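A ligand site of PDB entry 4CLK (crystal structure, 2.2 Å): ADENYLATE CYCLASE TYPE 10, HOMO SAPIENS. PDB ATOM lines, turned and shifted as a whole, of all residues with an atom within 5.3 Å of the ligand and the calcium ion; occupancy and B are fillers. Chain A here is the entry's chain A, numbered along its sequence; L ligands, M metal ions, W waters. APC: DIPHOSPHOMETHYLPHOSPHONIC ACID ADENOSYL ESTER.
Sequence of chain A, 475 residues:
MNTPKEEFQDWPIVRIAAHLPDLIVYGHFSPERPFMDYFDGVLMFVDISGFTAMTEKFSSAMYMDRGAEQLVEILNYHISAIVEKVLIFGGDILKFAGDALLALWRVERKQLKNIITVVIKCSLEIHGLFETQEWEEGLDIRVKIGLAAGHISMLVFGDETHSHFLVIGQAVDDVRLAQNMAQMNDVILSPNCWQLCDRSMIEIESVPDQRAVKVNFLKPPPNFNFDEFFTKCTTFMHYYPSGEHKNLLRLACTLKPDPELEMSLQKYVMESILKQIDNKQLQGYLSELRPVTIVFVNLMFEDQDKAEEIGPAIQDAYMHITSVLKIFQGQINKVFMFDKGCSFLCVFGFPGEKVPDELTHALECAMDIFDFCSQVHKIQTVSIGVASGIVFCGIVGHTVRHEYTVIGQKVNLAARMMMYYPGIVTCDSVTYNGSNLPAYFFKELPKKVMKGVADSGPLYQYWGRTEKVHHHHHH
The backbone NH (N) of Thr 52 is in hydrogen-bond range of an oxygen (O2G) of the ligand. The side-chain hydroxyl (OG1) of Thr 52 lies within hydrogen-bond range of an oxygen (O3G) of the ligand (2.6 Å). An oxygen (O2B) of the ligand lies within hydrogen-bond range of the side-chain hydroxyl of Ser 49 (2.6 Å). O of Val 406 lies within hydrogen-bond range of N6 of the ligand (2.7 Å). NH2 of Arg 416 is in salt-bridge range of O2A of the ligand (2.8 Å). O3G of the ligand is in hydrogen-bond range of ND2 of Asn 412, at 2.9 Å. The backbone NH (N) of Gly 50 lies within hydrogen-bond range of an oxygen (O2G) of the ligand, at 2.9 Å. An oxygen (O2G) of the ligand lies within hydrogen-bond range of the backbone NH (N) of Phe 51 (3.0 Å). The side-chain amino group (NZ) of Lys 144 is in salt-bridge range of an oxygen (O2B) of the ligand (3.7 Å).
The backbone carbonyl oxygen (O) of Asp 99 lies close to the backbone NH (N) of Ile 48 (3.2 Å). The side-chain carboxylate (OD2) of Asp 47 is in salt-bridge range of the side-chain amino group (NZ) of Lys 144, 3.3 Å away. OG1 of Thr 52 lies within hydrogen-bond range of ND2 of Asn 412 (3.5 Å). The side-chain hydroxyl of Ser 49 sits at hydrogen-bond distance from the side-chain amino group of Lys 144. N of Gly 98 lies within hydrogen-bond range of OG1 of Thr 405 (2.9 Å). The backbone carbonyl oxygen of Lys 334 lies within hydrogen-bond range of the backbone NH of Leu 345 (2.8 Å). The backbone carbonyl oxygen of Leu 345 is in hydrogen-bond range of the backbone NH of Asn 333 (2.6 Å). The side-chain amide nitrogen (ND2) of Asn 180 lies within hydrogen-bond range of the backbone carbonyl oxygen (O) of Arg 176 (3.3 Å).
The backbone NH of Gly 98 lies close to a nitrogen (N6) of the ligand, at 2.8 Å. Residues that only touch the ligand: Ala 97, Arg 176, Phe 296, Phe 336, Phe 338, Leu 345, Thr 405, Val 411 and Ala 415. Hydrophobic or aromatic side chains that line the ligand: Ala 97, Phe 296, Phe 336, Phe 338, Leu 345, Val 406, Val 411 and Ala 415. Of the 29 residues printed, 21 come within 4 Å of the ligand.
Within 4 Å of the calcium ion: Asp 47, Ile 48 and Asp 99. The nearest printed residue that does not touch the calcium ion is Ala 100 (4.5 Å).
The calcium ion is bound by OD1 of Asp 99 (2.3 Å). The calcium ion is bound by an oxygen (O1G) of the ligand (2.5 Å). OD1 of Asp 47 binds the calcium ion (2.5 Å). O1B of the ligand binds the calcium ion, at 2.7 Å. The calcium ion has four donor atoms within binding distance. Slightly farther from the calcium ion lies water W3 (3.0 Å). Slightly farther from the calcium ion lies O of Ile 48 (3.1 Å).
Water W3 bridges OD1 of Asn 412 and O3G of the ligand. Water W2 bridges N7 of the ligand (2.9 Å) and OD1 of Asn 412 (3.0 Å).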
ATOM      1  N   ASP A  47     -28.606  11.660 -33.258  1.00  0.00           N
ATOM      2  CA  ASP A  47     -28.319  10.875 -32.029  1.00  0.00           C
ATOM      3  C   ASP A  47     -28.241  11.765 -30.793  1.00  0.00           C
ATOM      4  O   ASP A  47     -27.505  12.722 -30.800  1.00  0.00           O
ATOM      5  CB  ASP A  47     -27.006  10.126 -32.188  1.00  0.00           C
ATOM      6  CG  ASP A  47     -26.586   9.376 -30.920  1.00  0.00           C
ATOM      7  OD1 ASP A  47     -27.449   8.636 -30.382  1.00  0.00           O
ATOM      8  OD2 ASP A  47     -25.416   9.542 -30.479  1.00  0.00           O
ATOM      9  N   ILE A  48     -28.978  11.476 -29.724  1.00  0.00           N
ATOM     10  CA  ILE A  48     -28.684  12.146 -28.430  1.00  0.00           C
ATOM     11  C   ILE A  48     -27.751  11.307 -27.542  1.00  0.00           C
ATOM     12  O   ILE A  48     -27.926  10.091 -27.386  1.00  0.00           O
ATOM     13  CB  ILE A  48     -29.922  12.480 -27.584  1.00  0.00           C
ATOM     14  CG1 ILE A  48     -30.969  13.272 -28.394  1.00  0.00           C
ATOM     15  CG2 ILE A  48     -29.484  13.258 -26.343  1.00  0.00           C
ATOM     16  CD1 ILE A  48     -30.686  14.741 -28.481  1.00  0.00           C
ATOM     17  N   SER A  49     -26.776  11.998 -26.968  1.00  0.00           N
ATOM     18  CA  SER A  49     -25.829  11.377 -26.087  1.00  0.00           C
ATOM     19  C   SER A  49     -26.071  11.979 -24.747  1.00  0.00           C
ATOM     20  O   SER A  49     -26.220  13.188 -24.644  1.00  0.00           O
ATOM     21  CB  SER A  49     -24.399  11.688 -26.525  1.00  0.00           C
ATOM     22  OG  SER A  49     -23.634  10.500 -26.578  1.00  0.00           O
ATOM     23  N   GLY A  50     -26.089  11.144 -23.714  1.00  0.00           N
ATOM     24  CA  GLY A  50     -26.239  11.589 -22.325  1.00  0.00           C
ATOM     25  C   GLY A  50     -27.467  11.007 -21.640  1.00  0.00           C
ATOM     26  O   GLY A  50     -27.615  11.113 -20.423  1.00  0.00           O
ATOM     27  N   PHE A  51     -28.325  10.362 -22.428  1.00  0.00           N
ATOM     28  CA  PHE A  51     -29.566   9.893 -21.885  1.00  0.00           C
ATOM     29  C   PHE A  51     -29.537   8.558 -21.212  1.00  0.00           C
ATOM     30  O   PHE A  51     -30.325   8.369 -20.306  1.00  0.00           O
ATOM     31  CB  PHE A  51     -30.713  10.032 -22.864  1.00  0.00           C
ATOM     32  CG  PHE A  51     -31.412  11.320 -22.687  1.00  0.00           C
ATOM     33  CD1 PHE A  51     -32.272  11.512 -21.615  1.00  0.00           C
ATOM     34  CD2 PHE A  51     -31.105  12.401 -23.509  1.00  0.00           C
ATOM     35  CE1 PHE A  51     -32.890  12.740 -21.401  1.00  0.00           C
ATOM     36  CE2 PHE A  51     -31.714  13.652 -23.315  1.00  0.00           C
ATOM     37  CZ  PHE A  51     -32.598  13.824 -22.255  1.00  0.00           C
ATOM     38  N   THR A  52     -28.661   7.626 -21.616  1.00  0.00           N
ATOM     39  CA  THR A  52     -28.611   6.321 -20.895  1.00  0.00           C
ATOM     40  C   THR A  52     -27.979   6.479 -19.499  1.00  0.00           C
ATOM     41  O   THR A  52     -28.213   5.673 -18.571  1.00  0.00           O
ATOM     42  CB  THR A  52     -27.938   5.192 -21.717  1.00  0.00           C
ATOM     43  OG1 THR A  52     -26.627   5.587 -22.073  1.00  0.00           O
ATOM     44  CG2 THR A  52     -28.710   4.931 -23.010  1.00  0.00           C
ATOM     45  N   ALA A  53     -27.208   7.567 -19.368  1.00  0.00           N
ATOM     46  CA  ALA A  53     -26.620   7.978 -18.097  1.00  0.00           C
ATOM     47  C   ALA A  53     -27.669   8.637 -17.198  1.00  0.00           C
ATOM     48  O   ALA A  53     -27.793   8.328 -16.012  1.00  0.00           O
ATOM     49  CB  ALA A  53     -25.476   8.935 -18.376  1.00  0.00           C
ATOM     50  N   ALA A  97     -35.356   5.305 -31.883  1.00  0.00           N
ATOM     51  CA  ALA A  97     -34.557   4.203 -31.351  1.00  0.00           C
ATOM     52  C   ALA A  97     -33.838   4.786 -30.124  1.00  0.00           C
ATOM     53  O   ALA A  97     -32.909   5.579 -30.228  1.00  0.00           O
ATOM     54  CB  ALA A  97     -33.555   3.746 -32.397  1.00  0.00           C
ATOM     55  N   GLY A  98     -34.392   4.487 -28.956  1.00  0.00           N
ATOM     56  CA  GLY A  98     -33.888   5.044 -27.732  1.00  0.00           C
ATOM     57  C   GLY A  98     -34.010   6.559 -27.780  1.00  0.00           C
ATOM     58  O   GLY A  98     -35.123   7.094 -27.839  1.00  0.00           O
ATOM     59  N   ASP A  99     -32.855   7.208 -27.757  1.00  0.00           N
ATOM     60  CA  ASP A  99     -32.746   8.677 -27.728  1.00  0.00           C
ATOM     61  C   ASP A  99     -32.314   9.276 -29.093  1.00  0.00           C
ATOM     62  O   ASP A  99     -31.944  10.470 -29.191  1.00  0.00           O
ATOM     63  CB  ASP A  99     -31.779   9.104 -26.585  1.00  0.00           C
ATOM     64  CG  ASP A  99     -30.458   8.297 -26.552  1.00  0.00           C
ATOM     65  OD1 ASP A  99     -30.221   7.474 -27.486  1.00  0.00           O
ATOM     66  OD2 ASP A  99     -29.683   8.471 -25.557  1.00  0.00           O
ATOM     67  N   ALA A 100     -32.364   8.442 -30.139  1.00  0.00           N
ATOM     68  CA  ALA A 100     -32.005   8.786 -31.502  1.00  0.00           C
ATOM     69  C   ALA A 100     -33.211   8.615 -32.414  1.00  0.00           C
ATOM     70  O   ALA A 100     -34.159   7.897 -32.089  1.00  0.00           O
ATOM     71  CB  ALA A 100     -30.907   7.870 -31.955  1.00  0.00           C
ATOM     72  N   LYS A 144     -25.359  14.442 -32.101  1.00  0.00           N
ATOM     73  CA  LYS A 144     -24.572  14.254 -33.302  1.00  0.00           C
ATOM     74  C   LYS A 144     -25.531  13.951 -34.432  1.00  0.00           C
ATOM     75  O   LYS A 144     -26.524  13.266 -34.245  1.00  0.00           O
ATOM     76  CB  LYS A 144     -23.586  13.119 -33.170  1.00  0.00           C
ATOM     77  CG  LYS A 144     -22.799  13.085 -31.882  1.00  0.00           C
ATOM     78  CD  LYS A 144     -21.808  11.940 -31.922  1.00  0.00           C
ATOM     79  CE  LYS A 144     -21.334  11.532 -30.535  1.00  0.00           C
ATOM     80  NZ  LYS A 144     -22.369  10.743 -29.826  1.00  0.00           N
ATOM     81  N   ARG A 176     -25.505   5.962 -40.847  1.00  0.00           N
ATOM     82  CA  ARG A 176     -25.030   5.473 -39.573  1.00  0.00           C
ATOM     83  C   ARG A 176     -23.540   5.684 -39.424  1.00  0.00           C
ATOM     84  O   ARG A 176     -23.091   6.207 -38.412  1.00  0.00           O
ATOM     85  CB  ARG A 176     -25.385   4.017 -39.311  1.00  0.00           C
ATOM     86  CG  ARG A 176     -25.208   3.700 -37.810  1.00  0.00           C
ATOM     87  CD  ARG A 176     -25.574   2.267 -37.394  1.00  0.00           C
ATOM     88  NE  ARG A 176     -27.009   2.081 -37.231  1.00  0.00           N
ATOM     89  CZ  ARG A 176     -27.713   2.371 -36.133  1.00  0.00           C
ATOM     90  NH1 ARG A 176     -27.127   2.883 -35.044  1.00  0.00           N
ATOM     91  NH2 ARG A 176     -29.017   2.148 -36.128  1.00  0.00           N
ATOM     92  N   GLN A 179     -22.866   9.334 -38.716  1.00  0.00           N
ATOM     93  CA  GLN A 179     -23.216   9.736 -37.357  1.00  0.00           C
ATOM     94  C   GLN A 179     -22.217   9.217 -36.290  1.00  0.00           C
ATOM     95  O   GLN A 179     -22.012   9.871 -35.290  1.00  0.00           O
ATOM     96  CB  GLN A 179     -24.654   9.307 -37.056  1.00  0.00           C
ATOM     97  CG  GLN A 179     -25.174   9.694 -35.683  1.00  0.00           C
ATOM     98  CD  GLN A 179     -24.829   8.659 -34.635  1.00  0.00           C
ATOM     99  OE1 GLN A 179     -24.783   7.452 -34.927  1.00  0.00           O
ATOM    100  NE2 GLN A 179     -24.526   9.111 -33.429  1.00  0.00           N
ATOM    101  N   ASN A 180     -21.620   8.070 -36.525  1.00  0.00           N
ATOM    102  CA  ASN A 180     -20.640   7.477 -35.617  1.00  0.00           C
ATOM    103  C   ASN A 180     -19.249   8.078 -35.694  1.00  0.00           C
ATOM    104  O   ASN A 180     -18.470   7.851 -34.781  1.00  0.00           O
ATOM    105  CB  ASN A 180     -20.532   5.972 -35.862  1.00  0.00           C
ATOM    106  CG  ASN A 180     -21.732   5.217 -35.347  1.00  0.00           C
ATOM    107  OD1 ASN A 180     -22.321   5.583 -34.318  1.00  0.00           O
ATOM    108  ND2 ASN A 180     -22.112   4.154 -36.035  1.00  0.00           N
ATOM    109  N   PHE A 296     -31.216  -8.948 -27.900  1.00  0.00           N
ATOM    110  CA  PHE A 296     -30.899  -8.200 -29.117  1.00  0.00           C
ATOM    111  C   PHE A 296     -30.333  -9.110 -30.176  1.00  0.00           C
ATOM    112  O   PHE A 296     -29.191  -9.551 -30.020  1.00  0.00           O
ATOM    113  CB  PHE A 296     -29.855  -7.128 -28.821  1.00  0.00           C
ATOM    114  CG  PHE A 296     -30.171  -5.786 -29.402  1.00  0.00           C
ATOM    115  CD1 PHE A 296     -30.568  -5.646 -30.731  1.00  0.00           C
ATOM    116  CD2 PHE A 296     -30.079  -4.642 -28.598  1.00  0.00           C
ATOM    117  CE1 PHE A 296     -30.879  -4.376 -31.258  1.00  0.00           C
ATOM    118  CE2 PHE A 296     -30.390  -3.389 -29.115  1.00  0.00           C
ATOM    119  CZ  PHE A 296     -30.814  -3.262 -30.445  1.00  0.00           C
ATOM    120  N   ASN A 333     -39.554  -4.958 -29.981  1.00  0.00           N
ATOM    121  CA  ASN A 333     -39.761  -3.519 -29.805  1.00  0.00           C
ATOM    122  C   ASN A 333     -39.402  -2.702 -31.025  1.00  0.00           C
ATOM    123  O   ASN A 333     -40.001  -1.696 -31.254  1.00  0.00           O
ATOM    124  CB  ASN A 333     -38.963  -2.984 -28.601  1.00  0.00           C
ATOM    125  CG  ASN A 333     -38.952  -1.435 -28.516  1.00  0.00           C
ATOM    126  OD1 ASN A 333     -37.985  -0.770 -28.889  1.00  0.00           O
ATOM    127  ND2 ASN A 333     -40.036  -0.875 -28.031  1.00  0.00           N
ATOM    128  N   LYS A 334     -38.362  -3.103 -31.767  1.00  0.00           N
ATOM    129  CA  LYS A 334     -37.922  -2.371 -32.934  1.00  0.00           C
ATOM    130  C   LYS A 334     -37.112  -3.281 -33.819  1.00  0.00           C
ATOM    131  O   LYS A 334     -36.405  -4.188 -33.332  1.00  0.00           O
ATOM    132  CB  LYS A 334     -36.912  -1.274 -32.577  1.00  0.00           C
ATOM    133  CG  LYS A 334     -37.423  -0.064 -31.872  1.00  0.00           C
ATOM    134  CD  LYS A 334     -38.396   0.814 -32.676  1.00  0.00           C
ATOM    135  CE  LYS A 334     -39.162   1.619 -31.636  1.00  0.00           C
ATOM    136  NZ  LYS A 334     -40.151   2.520 -32.228  1.00  0.00           N
ATOM    137  N   PHE A 336     -34.277  -2.756 -37.149  1.00  0.00           N
ATOM    138  CA  PHE A 336     -33.530  -1.774 -37.906  1.00  0.00           C
ATOM    139  C   PHE A 336     -32.204  -2.351 -38.380  1.00  0.00           C
ATOM    140  O   PHE A 336     -31.670  -3.255 -37.753  1.00  0.00           O
ATOM    141  CB  PHE A 336     -33.312  -0.510 -37.057  1.00  0.00           C
ATOM    142  CG  PHE A 336     -32.607  -0.764 -35.783  1.00  0.00           C
ATOM    143  CD1 PHE A 336     -33.304  -1.132 -34.652  1.00  0.00           C
ATOM    144  CD2 PHE A 336     -31.222  -0.660 -35.715  1.00  0.00           C
ATOM    145  CE1 PHE A 336     -32.646  -1.368 -33.464  1.00  0.00           C
ATOM    146  CE2 PHE A 336     -30.543  -0.880 -34.538  1.00  0.00           C
ATOM    147  CZ  PHE A 336     -31.253  -1.250 -33.411  1.00  0.00           C
ATOM    148  N   PHE A 338     -28.326  -2.293 -38.592  1.00  0.00           N
ATOM    149  CA  PHE A 338     -27.152  -1.845 -37.840  1.00  0.00           C
ATOM    150  C   PHE A 338     -26.013  -1.604 -38.836  1.00  0.00           C
ATOM    151  O   PHE A 338     -26.247  -1.569 -40.048  1.00  0.00           O
ATOM    152  CB  PHE A 338     -26.750  -2.909 -36.799  1.00  0.00           C
ATOM    153  CG  PHE A 338     -26.553  -2.363 -35.419  1.00  0.00           C
ATOM    154  CD1 PHE A 338     -25.304  -1.902 -34.994  1.00  0.00           C
ATOM    155  CD2 PHE A 338     -27.613  -2.334 -34.519  1.00  0.00           C
ATOM    156  CE1 PHE A 338     -25.135  -1.413 -33.708  1.00  0.00           C
ATOM    157  CE2 PHE A 338     -27.444  -1.845 -33.233  1.00  0.00           C
ATOM    158  CZ  PHE A 338     -26.196  -1.387 -32.832  1.00  0.00           C
ATOM    159  N   LEU A 345     -34.818  -5.811 -31.715  1.00  0.00           N
ATOM    160  CA  LEU A 345     -34.679  -5.481 -30.325  1.00  0.00           C
ATOM    161  C   LEU A 345     -35.905  -6.023 -29.613  1.00  0.00           C
ATOM    162  O   LEU A 345     -36.996  -5.446 -29.698  1.00  0.00           O
ATOM    163  CB  LEU A 345     -34.504  -3.985 -30.154  1.00  0.00           C
ATOM    164  CG  LEU A 345     -34.031  -3.457 -28.786  1.00  0.00           C
ATOM    165  CD1 LEU A 345     -33.914  -1.943 -28.816  1.00  0.00           C
ATOM    166  CD2 LEU A 345     -34.944  -3.854 -27.682  1.00  0.00           C
ATOM    167  N   THR A 405     -40.518   3.315 -26.831  1.00  0.00           N
ATOM    168  CA  THR A 405     -39.117   2.921 -26.928  1.00  0.00           C
ATOM    169  C   THR A 405     -38.551   2.466 -25.560  1.00  0.00           C
ATOM    170  O   THR A 405     -39.207   2.584 -24.496  1.00  0.00           O
ATOM    171  CB  THR A 405     -38.301   4.051 -27.633  1.00  0.00           C
ATOM    172  OG1 THR A 405     -37.017   3.545 -28.068  1.00  0.00           O
ATOM    173  CG2 THR A 405     -38.042   5.135 -26.755  1.00  0.00           C
ATOM    174  N   VAL A 406     -37.363   1.874 -25.597  1.00  0.00           N
ATOM    175  CA  VAL A 406     -36.627   1.512 -24.385  1.00  0.00           C
ATOM    176  C   VAL A 406     -35.258   2.193 -24.388  1.00  0.00           C
ATOM    177  O   VAL A 406     -34.682   2.375 -25.419  1.00  0.00           O
ATOM    178  CB  VAL A 406     -36.451   0.013 -24.234  1.00  0.00           C
ATOM    179  CG1 VAL A 406     -37.801  -0.616 -24.127  1.00  0.00           C
ATOM    180  CG2 VAL A 406     -35.705  -0.559 -25.430  1.00  0.00           C
ATOM    181  N   ILE A 407     -34.809   2.594 -23.208  1.00  0.00           N
ATOM    182  CA  ILE A 407     -33.597   3.328 -23.046  1.00  0.00           C
ATOM    183  C   ILE A 407     -32.951   2.837 -21.776  1.00  0.00           C
ATOM    184  O   ILE A 407     -33.599   2.762 -20.721  1.00  0.00           O
ATOM    185  CB  ILE A 407     -33.844   4.833 -22.897  1.00  0.00           C
ATOM    186  CG1 ILE A 407     -34.579   5.368 -24.094  1.00  0.00           C
ATOM    187  CG2 ILE A 407     -32.531   5.586 -22.800  1.00  0.00           C
ATOM    188  CD1 ILE A 407     -34.892   6.861 -24.002  1.00  0.00           C
ATOM    189  N   VAL A 411     -29.660  -1.865 -22.561  1.00  0.00           N
ATOM    190  CA  VAL A 411     -30.034  -1.912 -23.966  1.00  0.00           C
ATOM    191  C   VAL A 411     -28.779  -1.790 -24.792  1.00  0.00           C
ATOM    192  O   VAL A 411     -28.568  -2.581 -25.729  1.00  0.00           O
ATOM    193  CB  VAL A 411     -31.081  -0.795 -24.356  1.00  0.00           C
ATOM    194  CG1 VAL A 411     -31.490  -0.936 -25.802  1.00  0.00           C
ATOM    195  CG2 VAL A 411     -32.361  -0.889 -23.504  1.00  0.00           C
ATOM    196  N   ASN A 412     -27.965  -0.788 -24.476  1.00  0.00           N
ATOM    197  CA  ASN A 412     -26.679  -0.603 -25.158  1.00  0.00           C
ATOM    198  C   ASN A 412     -25.748  -1.822 -24.993  1.00  0.00           C
ATOM    199  O   ASN A 412     -25.071  -2.219 -25.940  1.00  0.00           O
ATOM    200  CB  ASN A 412     -25.916   0.640 -24.618  1.00  0.00           C
ATOM    201  CG  ASN A 412     -26.668   1.943 -24.819  1.00  0.00           C
ATOM    202  OD1 ASN A 412     -27.796   1.994 -25.327  1.00  0.00           O
ATOM    203  ND2 ASN A 412     -26.043   3.024 -24.371  1.00  0.00           N
ATOM    204  N   ALA A 415     -26.758  -4.652 -27.242  1.00  0.00           N
ATOM    205  CA  ALA A 415     -26.339  -4.233 -28.596  1.00  0.00           C
ATOM    206  C   ALA A 415     -24.820  -4.363 -28.798  1.00  0.00           C
ATOM    207  O   ALA A 415     -24.386  -4.903 -29.806  1.00  0.00           O
ATOM    208  CB  ALA A 415     -26.764  -2.790 -28.896  1.00  0.00           C
ATOM    209  N   ARG A 416     -24.007  -3.849 -27.859  1.00  0.00           N
ATOM    210  CA  ARG A 416     -22.553  -3.997 -27.994  1.00  0.00           C
ATOM    211  C   ARG A 416     -22.112  -5.449 -27.940  1.00  0.00           C
ATOM    212  O   ARG A 416     -21.166  -5.793 -28.627  1.00  0.00           O
ATOM    213  CB  ARG A 416     -21.721  -3.191 -26.978  1.00  0.00           C
ATOM    214  CG  ARG A 416     -21.881  -1.667 -26.992  1.00  0.00           C
ATOM    215  CD  ARG A 416     -22.153  -1.091 -28.373  1.00  0.00           C
ATOM    216  NE  ARG A 416     -21.923   0.373 -28.449  1.00  0.00           N
ATOM    217  CZ  ARG A 416     -21.815   1.071 -29.592  1.00  0.00           C
ATOM    218  NH1 ARG A 416     -21.936   0.485 -30.769  1.00  0.00           N
ATOM    219  NH2 ARG A 416     -21.588   2.389 -29.562  1.00  0.00           N
ATOM    220  N   LYS A 451     -17.192   0.010 -27.006  1.00  0.00           N
ATOM    221  CA  LYS A 451     -17.559   1.444 -27.205  1.00  0.00           C
ATOM    222  C   LYS A 451     -18.842   1.841 -26.488  1.00  0.00           C
ATOM    223  O   LYS A 451     -19.935   1.376 -26.825  1.00  0.00           O
ATOM    224  CB  LYS A 451     -17.680   1.823 -28.700  1.00  0.00           C
HETATM  225  PG  APC L   1     -26.464   7.342 -24.945  1.00  0.00           P
HETATM  226  O1G APC L   1     -27.490   7.502 -26.044  1.00  0.00           O
HETATM  227  O2G APC L   1     -26.669   8.274 -23.775  1.00  0.00           O
HETATM  228  O3G APC L   1     -26.191   5.912 -24.565  1.00  0.00           O
HETATM  229  PB  APC L   1     -24.705   7.508 -27.128  1.00  0.00           P
HETATM  230  O1B APC L   1     -25.629   8.129 -28.104  1.00  0.00           O
HETATM  231  O2B APC L   1     -23.217   8.093 -27.327  1.00  0.00           O
HETATM  232  O3B APC L   1     -25.137   7.928 -25.643  1.00  0.00           O
HETATM  233  PA  APC L   1     -24.552   4.908 -28.848  1.00  0.00           P
HETATM  234  O1A APC L   1     -25.224   5.541 -29.999  1.00  0.00           O
HETATM  235  O2A APC L   1     -22.964   4.763 -29.113  1.00  0.00           O
HETATM  236  C3A APC L   1     -24.830   5.688 -27.215  1.00  0.00           C
HETATM  237  O5' APC L   1     -25.368   3.538 -28.711  1.00  0.00           O
HETATM  238  C5' APC L   1     -24.892   2.246 -28.375  1.00  0.00           C
HETATM  239  C4' APC L   1     -25.784   1.312 -29.178  1.00  0.00           C
HETATM  240  O4' APC L   1     -26.932   0.953 -28.414  1.00  0.00           O
HETATM  241  C3' APC L   1     -26.298   1.940 -30.472  1.00  0.00           C
HETATM  242  O3' APC L   1     -25.526   1.444 -31.543  1.00  0.00           O
HETATM  243  C2' APC L   1     -27.751   1.535 -30.593  1.00  0.00           C
HETATM  244  O2' APC L   1     -28.021   0.828 -31.814  1.00  0.00           O
HETATM  245  C1' APC L   1     -28.019   0.693 -29.338  1.00  0.00           C
HETATM  246  N9  APC L   1     -29.326   1.054 -28.718  1.00  0.00           N
HETATM  247  C8  APC L   1     -29.531   1.481 -27.456  1.00  0.00           C
HETATM  248  N7  APC L   1     -30.852   1.734 -27.205  1.00  0.00           N
HETATM  249  C5  APC L   1     -31.511   1.459 -28.350  1.00  0.00           C
HETATM  250  C6  APC L   1     -32.928   1.503 -28.810  1.00  0.00           C
HETATM  251  N6  APC L   1     -33.944   1.855 -28.014  1.00  0.00           N
HETATM  252  N1  APC L   1     -33.183   1.137 -30.086  1.00  0.00           N
HETATM  253  C2  APC L   1     -32.196   0.758 -30.927  1.00  0.00           C
HETATM  254  N3  APC L   1     -30.888   0.682 -30.577  1.00  0.00           N
HETATM  255  C4  APC L   1     -30.496   1.017 -29.332  1.00  0.00           C
HETATM  256 CA    CA M   1     -28.128   7.152 -28.449  1.00  0.00          CA
HETATM  257  O   HOH W   1     -30.410   4.301 -30.205  1.00  0.00           O
HETATM  258  O   HOH W   2     -30.554   2.878 -24.533  1.00  0.00           O
HETATM  259  O   HOH W   3     -28.664   4.871 -26.597  1.00  0.00           O
